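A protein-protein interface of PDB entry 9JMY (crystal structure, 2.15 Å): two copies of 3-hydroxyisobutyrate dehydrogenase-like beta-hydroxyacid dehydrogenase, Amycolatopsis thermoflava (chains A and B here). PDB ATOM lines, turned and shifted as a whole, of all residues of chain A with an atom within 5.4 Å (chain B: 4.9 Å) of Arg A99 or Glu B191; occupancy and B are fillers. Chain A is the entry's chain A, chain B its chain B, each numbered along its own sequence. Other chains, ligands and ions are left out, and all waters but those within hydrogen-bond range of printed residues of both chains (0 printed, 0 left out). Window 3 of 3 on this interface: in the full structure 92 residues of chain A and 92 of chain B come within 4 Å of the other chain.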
ATOM      1  N   THR A  94       2.666 -21.318  -4.416  1.00  0.00           N
ATOM      2  CA  THR A  94       2.153 -20.179  -3.615  1.00  0.00           C
ATOM      3  C   THR A  94       0.770 -20.552  -3.118  1.00  0.00           C
ATOM      4  O   THR A  94       0.056 -21.328  -3.760  1.00  0.00           O
ATOM      5  CB  THR A  94       2.096 -18.854  -4.400  1.00  0.00           C
ATOM      6  OG1 THR A  94       1.089 -18.920  -5.408  1.00  0.00           O
ATOM      7  CG2 THR A  94       3.401 -18.486  -5.061  1.00  0.00           C
ATOM      8  N   PRO A  95       0.338 -19.958  -1.988  1.00  0.00           N
ATOM      9  CA  PRO A  95      -1.040 -20.109  -1.523  1.00  0.00           C
ATOM     10  C   PRO A  95      -2.087 -19.724  -2.591  1.00  0.00           C
ATOM     11  O   PRO A  95      -3.041 -20.461  -2.786  1.00  0.00           O
ATOM     12  CB  PRO A  95      -1.054 -19.176  -0.299  1.00  0.00           C
ATOM     13  CG  PRO A  95       0.364 -19.255   0.187  1.00  0.00           C
ATOM     14  CD  PRO A  95       1.162 -19.149  -1.091  1.00  0.00           C
ATOM     15  N   GLN A  96      -1.900 -18.584  -3.253  1.00  0.00           N
ATOM     16  CA  GLN A  96      -2.791 -18.112  -4.353  1.00  0.00           C
ATOM     17  C   GLN A  96      -2.863 -19.189  -5.445  1.00  0.00           C
ATOM     18  O   GLN A  96      -3.977 -19.558  -5.835  1.00  0.00           O
ATOM     19  CB  GLN A  96      -2.365 -16.733  -4.876  1.00  0.00           C
ATOM     20  CG  GLN A  96      -2.676 -16.455  -6.353  1.00  0.00           C
ATOM     21  CD  GLN A  96      -4.140 -16.522  -6.727  1.00  0.00           C
ATOM     22  OE1 GLN A  96      -5.013 -16.725  -5.882  1.00  0.00           O
ATOM     23  NE2 GLN A  96      -4.429 -16.357  -8.014  1.00  0.00           N
ATOM     24  N   ARG A  97      -1.738 -19.714  -5.918  1.00  0.00           N
ATOM     25  CA  ARG A  97      -1.785 -20.699  -7.026  1.00  0.00           C
ATOM     26  C   ARG A  97      -2.471 -21.986  -6.549  1.00  0.00           C
ATOM     27  O   ARG A  97      -3.124 -22.646  -7.374  1.00  0.00           O
ATOM     28  CB  ARG A  97      -0.394 -20.878  -7.630  1.00  0.00           C
ATOM     29  CG  ARG A  97       0.034 -19.695  -8.489  1.00  0.00           C
ATOM     30  CD  ARG A  97       0.467 -20.124  -9.869  1.00  0.00           C
ATOM     31  NE  ARG A  97       1.555 -21.105  -9.808  1.00  0.00           N
ATOM     32  CZ  ARG A  97       1.877 -21.983 -10.768  1.00  0.00           C
ATOM     33  NH1 ARG A  97       1.184 -21.999 -11.892  1.00  0.00           N
ATOM     34  NH2 ARG A  97       2.894 -22.835 -10.603  1.00  0.00           N
ATOM     35  N   THR A  98      -2.362 -22.328  -5.261  1.00  0.00           N
ATOM     36  CA  THR A  98      -2.997 -23.539  -4.692  1.00  0.00           C
ATOM     37  C   THR A  98      -4.518 -23.335  -4.670  1.00  0.00           C
ATOM     38  O   THR A  98      -5.257 -24.306  -4.944  1.00  0.00           O
ATOM     39  CB  THR A  98      -2.458 -23.837  -3.286  1.00  0.00           C
ATOM     40  OG1 THR A  98      -1.032 -23.886  -3.389  1.00  0.00           O
ATOM     41  CG2 THR A  98      -3.010 -25.129  -2.727  1.00  0.00           C
ATOM     42  N   ARG A  99      -4.954 -22.134  -4.289  1.00  0.00           N
ATOM     43  CA  ARG A  99      -6.384 -21.735  -4.233  1.00  0.00           C
ATOM     44  C   ARG A  99      -6.972 -21.755  -5.649  1.00  0.00           C
ATOM     45  O   ARG A  99      -8.051 -22.321  -5.842  1.00  0.00           O
ATOM     46  CB  ARG A  99      -6.501 -20.370  -3.556  1.00  0.00           C
ATOM     47  CG  ARG A  99      -6.317 -20.426  -2.044  1.00  0.00           C
ATOM     48  CD  ARG A  99      -6.179 -19.039  -1.444  1.00  0.00           C
ATOM     49  NE  ARG A  99      -5.858 -19.064  -0.026  1.00  0.00           N
ATOM     50  CZ  ARG A  99      -4.918 -18.339   0.590  1.00  0.00           C
ATOM     51  NH1 ARG A  99      -4.150 -17.485  -0.067  1.00  0.00           N
ATOM     52  NH2 ARG A  99      -4.753 -18.461   1.896  1.00  0.00           N
ATOM     53  N   GLU A 100      -6.258 -21.212  -6.628  1.00  0.00           N
ATOM     54  CA  GLU A 100      -6.741 -21.155  -8.031  1.00  0.00           C
ATOM     55  C   GLU A 100      -6.783 -22.607  -8.564  1.00  0.00           C
ATOM     56  O   GLU A 100      -7.806 -22.985  -9.180  1.00  0.00           O
ATOM     57  CB  GLU A 100      -5.936 -20.109  -8.819  1.00  0.00           C
ATOM     58  CG  GLU A 100      -4.760 -20.658  -9.602  1.00  0.00           C
ATOM     59  CD  GLU A 100      -4.027 -19.636 -10.458  1.00  0.00           C
ATOM     60  OE1 GLU A 100      -3.159 -20.043 -11.253  1.00  0.00           O
ATOM     61  OE2 GLU A 100      -4.318 -18.437 -10.324  1.00  0.00           O
ATOM     62  N   ALA A 101      -5.795 -23.442  -8.232  1.00  0.00           N
ATOM     63  CA  ALA A 101      -5.803 -24.890  -8.542  1.00  0.00           C
ATOM     64  C   ALA A 101      -7.063 -25.578  -7.989  1.00  0.00           C
ATOM     65  O   ALA A 101      -7.578 -26.490  -8.662  1.00  0.00           O
ATOM     66  CB  ALA A 101      -4.549 -25.543  -8.023  1.00  0.00           C
ATOM     67  N   ALA A 102      -7.548 -25.189  -6.812  1.00  0.00           N
ATOM     68  CA  ALA A 102      -8.746 -25.805  -6.195  1.00  0.00           C
ATOM     69  C   ALA A 102      -9.957 -25.557  -7.114  1.00  0.00           C
ATOM     70  O   ALA A 102     -10.726 -26.511  -7.365  1.00  0.00           O
ATOM     71  CB  ALA A 102      -8.975 -25.259  -4.807  1.00  0.00           C
ATOM     72  N   ALA A 103     -10.106 -24.310  -7.582  1.00  0.00           N
ATOM     73  CA  ALA A 103     -11.177 -23.827  -8.489  1.00  0.00           C
ATOM     74  C   ALA A 103     -11.173 -24.651  -9.774  1.00  0.00           C
ATOM     75  O   ALA A 103     -12.229 -25.220 -10.134  1.00  0.00           O
ATOM     76  CB  ALA A 103     -10.947 -22.369  -8.783  1.00  0.00           C
ATOM     77  N   ASP A 159      -9.697 -23.637   3.930  1.00  0.00           N
ATOM     78  CA  ASP A 159      -8.923 -22.853   2.930  1.00  0.00           C
ATOM     79  C   ASP A 159      -7.803 -23.747   2.379  1.00  0.00           C
ATOM     80  O   ASP A 159      -6.896 -24.080   3.148  1.00  0.00           O
ATOM     81  CB  ASP A 159      -8.393 -21.536   3.522  1.00  0.00           C
ATOM     82  CG  ASP A 159      -7.409 -20.819   2.611  1.00  0.00           C
ATOM     83  OD1 ASP A 159      -7.350 -21.158   1.427  1.00  0.00           O
ATOM     84  OD2 ASP A 159      -6.652 -19.972   3.099  1.00  0.00           O
ATOM     85  N   HIS A 160      -7.835 -24.059   1.080  1.00  0.00           N
ATOM     86  CA  HIS A 160      -6.842 -24.915   0.362  1.00  0.00           C
ATOM     87  C   HIS A 160      -5.431 -24.299   0.435  1.00  0.00           C
ATOM     88  O   HIS A 160      -4.454 -25.049   0.350  1.00  0.00           O
ATOM     89  CB  HIS A 160      -7.263 -25.124  -1.099  1.00  0.00           C
ATOM     90  CG  HIS A 160      -8.601 -25.765  -1.294  1.00  0.00           C
ATOM     91  ND1 HIS A 160      -9.791 -25.057  -1.219  1.00  0.00           N
ATOM     92  CD2 HIS A 160      -8.941 -27.039  -1.607  1.00  0.00           C
ATOM     93  CE1 HIS A 160     -10.803 -25.874  -1.472  1.00  0.00           C
ATOM     94  NE2 HIS A 160     -10.308 -27.098  -1.701  1.00  0.00           N
ATOM     95  N   GLY A 161      -5.327 -22.971   0.561  1.00  0.00           N
ATOM     96  CA  GLY A 161      -4.047 -22.243   0.636  1.00  0.00           C
ATOM     97  C   GLY A 161      -3.370 -22.309   2.006  1.00  0.00           C
ATOM     98  O   GLY A 161      -2.203 -21.908   2.067  1.00  0.00           O
ATOM     99  N   LEU A 162      -4.015 -22.820   3.057  1.00  0.00           N
ATOM    100  CA  LEU A 162      -3.431 -22.874   4.431  1.00  0.00           C
ATOM    101  C   LEU A 162      -2.250 -23.842   4.497  1.00  0.00           C
ATOM    102  O   LEU A 162      -1.152 -23.408   4.929  1.00  0.00           O
ATOM    103  CB  LEU A 162      -4.494 -23.278   5.451  1.00  0.00           C
ATOM    104  CG  LEU A 162      -5.292 -22.128   6.038  1.00  0.00           C
ATOM    105  CD1 LEU A 162      -6.569 -22.648   6.673  1.00  0.00           C
ATOM    106  CD2 LEU A 162      -4.458 -21.341   7.034  1.00  0.00           C
ATOM    107  N   LEU A 165       0.554 -22.347   2.753  1.00  0.00           N
ATOM    108  CA  LEU A 165       1.048 -21.163   3.516  1.00  0.00           C
ATOM    109  C   LEU A 165       1.994 -21.633   4.635  1.00  0.00           C
ATOM    110  O   LEU A 165       3.091 -21.074   4.776  1.00  0.00           O
ATOM    111  CB  LEU A 165      -0.166 -20.421   4.087  1.00  0.00           C
ATOM    112  CG  LEU A 165       0.135 -19.263   5.027  1.00  0.00           C
ATOM    113  CD1 LEU A 165       1.031 -18.237   4.335  1.00  0.00           C
ATOM    114  CD2 LEU A 165      -1.169 -18.628   5.498  1.00  0.00           C
ATOM    115  N   ALA B 186       5.695 -13.165   9.165  1.00  0.00           N
ATOM    116  CA  ALA B 186       5.172 -12.077   8.317  1.00  0.00           C
ATOM    117  C   ALA B 186       4.286 -12.672   7.221  1.00  0.00           C
ATOM    118  O   ALA B 186       3.188 -12.137   6.981  1.00  0.00           O
ATOM    119  CB  ALA B 186       6.294 -11.283   7.730  1.00  0.00           C
ATOM    120  N   LEU B 187       4.758 -13.721   6.549  1.00  0.00           N
ATOM    121  CA  LEU B 187       3.966 -14.372   5.487  1.00  0.00           C
ATOM    122  C   LEU B 187       2.612 -14.792   6.091  1.00  0.00           C
ATOM    123  O   LEU B 187       1.569 -14.400   5.524  1.00  0.00           O
ATOM    124  CB  LEU B 187       4.780 -15.537   4.927  1.00  0.00           C
ATOM    125  CG  LEU B 187       4.119 -16.346   3.818  1.00  0.00           C
ATOM    126  CD1 LEU B 187       3.692 -15.451   2.655  1.00  0.00           C
ATOM    127  CD2 LEU B 187       5.068 -17.435   3.327  1.00  0.00           C
ATOM    128  N   LEU B 188       2.622 -15.480   7.240  1.00  0.00           N
ATOM    129  CA  LEU B 188       1.402 -15.968   7.927  1.00  0.00           C
ATOM    130  C   LEU B 188       0.507 -14.777   8.293  1.00  0.00           C
ATOM    131  O   LEU B 188      -0.683 -14.857   8.023  1.00  0.00           O
ATOM    132  CB  LEU B 188       1.769 -16.740   9.202  1.00  0.00           C
ATOM    133  CG  LEU B 188       2.275 -18.182   9.070  1.00  0.00           C
ATOM    134  CD1 LEU B 188       1.382 -19.155   9.813  1.00  0.00           C
ATOM    135  CD2 LEU B 188       2.462 -18.630   7.647  1.00  0.00           C
ATOM    136  N   ALA B 189       1.063 -13.757   8.947  1.00  0.00           N
ATOM    137  CA  ALA B 189       0.324 -12.579   9.448  1.00  0.00           C
ATOM    138  C   ALA B 189      -0.283 -11.809   8.260  1.00  0.00           C
ATOM    139  O   ALA B 189      -1.418 -11.380   8.369  1.00  0.00           O
ATOM    140  CB  ALA B 189       1.233 -11.705  10.289  1.00  0.00           C
ATOM    141  N   ALA B 190       0.428 -11.685   7.146  1.00  0.00           N
ATOM    142  CA  ALA B 190      -0.048 -10.947   5.951  1.00  0.00           C
ATOM    143  C   ALA B 190      -1.243 -11.692   5.345  1.00  0.00           C
ATOM    144  O   ALA B 190      -2.151 -11.016   4.830  1.00  0.00           O
ATOM    145  CB  ALA B 190       1.075 -10.768   4.965  1.00  0.00           C
ATOM    146  N   GLU B 191      -1.265 -13.032   5.462  1.00  0.00           N
ATOM    147  CA  GLU B 191      -2.322 -13.906   4.895  1.00  0.00           C
ATOM    148  C   GLU B 191      -3.461 -14.131   5.896  1.00  0.00           C
ATOM    149  O   GLU B 191      -4.337 -14.941   5.586  1.00  0.00           O
ATOM    150  CB  GLU B 191      -1.746 -15.271   4.504  1.00  0.00           C
ATOM    151  CG  GLU B 191      -0.820 -15.235   3.315  1.00  0.00           C
ATOM    152  CD  GLU B 191      -1.490 -15.275   1.952  1.00  0.00           C
ATOM    153  OE1 GLU B 191      -1.010 -14.561   1.055  1.00  0.00           O
ATOM    154  OE2 GLU B 191      -2.476 -16.033   1.782  1.00  0.00           O
ATOM    155  N   GLY B 192      -3.452 -13.498   7.066  1.00  0.00           N
ATOM    156  CA  GLY B 192      -4.545 -13.634   8.049  1.00  0.00           C
ATOM    157  C   GLY B 192      -4.311 -14.737   9.066  1.00  0.00           C
ATOM    158  O   GLY B 192      -5.086 -14.837  10.009  1.00  0.00           O
ATOM    159  N   ALA B 193      -3.267 -15.544   8.907  1.00  0.00           N
ATOM    160  CA  ALA B 193      -2.991 -16.698   9.789  1.00  0.00           C
ATOM    161  C   ALA B 193      -2.243 -16.204  11.019  1.00  0.00           C
ATOM    162  O   ALA B 193      -1.553 -15.177  10.936  1.00  0.00           O
ATOM    163  CB  ALA B 193      -2.191 -17.728   9.045  1.00  0.00           C
ATOM    164  N   ALA B 245       5.170 -15.814  -2.872  1.00  0.00           N
ATOM    165  CA  ALA B 245       4.152 -15.835  -1.789  1.00  0.00           C
ATOM    166  C   ALA B 245       4.312 -14.562  -0.953  1.00  0.00           C
ATOM    167  O   ALA B 245       3.292 -13.903  -0.638  1.00  0.00           O
ATOM    168  CB  ALA B 245       4.316 -17.087  -0.954  1.00  0.00           C
ATOM    169  N   ALA B 249       1.814 -11.339  -0.673  1.00  0.00           N
ATOM    170  CA  ALA B 249       1.323 -10.955   0.674  1.00  0.00           C
ATOM    171  C   ALA B 249       1.792  -9.540   1.072  1.00  0.00           C
ATOM    172  O   ALA B 249       1.276  -8.998   2.044  1.00  0.00           O
ATOM    173  CB  ALA B 249       1.758 -12.013   1.659  1.00  0.00           C
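The side-chain hydroxyl of Thr A94 lies within hydrogen-bond range of the backbone NH of Arg A97, 3.0 Å away. The guanidinium group (NH2) of Arg A99 lies within salt-bridge range of the side-chain carboxylate (OD2) of Asp A159, 2.7 Å away. The backbone carbonyl oxygen (O) of Leu B188 is in hydrogen-bond range of the backbone NH (N) of Ala B193 (2.8 Å). The side-chain hydroxyl (OG1) of Thr A98 is in hydrogen-bond range of the backbone carbonyl oxygen (O) of Thr A94 (2.8 Å).
Printed residues of chain B within 4 Å of Pro A95: Ala B245 (3.8 Å). Of chain B, only Glu B191 comes within 4 Å of Arg A99. Of the printed residues of chain A, Leu B187 touches Leu A165 (3.7 Å). Glu B191 touches just these residues of chain A: Arg A99 (2.9 Å) and Leu A165 (3.5 Å). Gly B192 touches none of the printed residues of chain A. Of the printed residues of chain A, Ala B245 touches Thr A94 and Pro A95. The nearest printed residue of chain B that does not touch Arg A99 is Gly B192 (7.3 Å). The nearest residue of chain A that does not touch Glu B191 is Pro A95 (4.03 Å).
Hydrophobic or aromatic side chains of chain B within 4 Å of the printed part of chain A: Leu B187, Leu B188, Ala B193 and Ala B245. Printed residues of chain A that touch a printed residue of chain B: Thr A94, Pro A95, Arg A99 and Leu A165. Hydrophobic or aromatic side chains of chain A within 4 Å of the printed part of chain B: Pro A95 and Leu A165. Among the printed residues, 7 pairs touch across the chains.
Thr A94 touches Ala B245 (CG2 to N, 3.9 Å). Ala B245 touches Pro A95. Leu B187 touches Leu A165 (CG to CD1, 3.7 Å). Leu A165 touches Leu B188. Leu A165 touches Glu B191. Ala B193 touches Leu A165 (CB to CD2, 3.8 Å).
No position is printed for both chains.
The side-chain carboxylate (OE2) of Glu B191 lies within salt-bridge range of the guanidinium group (NH1) of Arg A99, at 2.9 Å.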
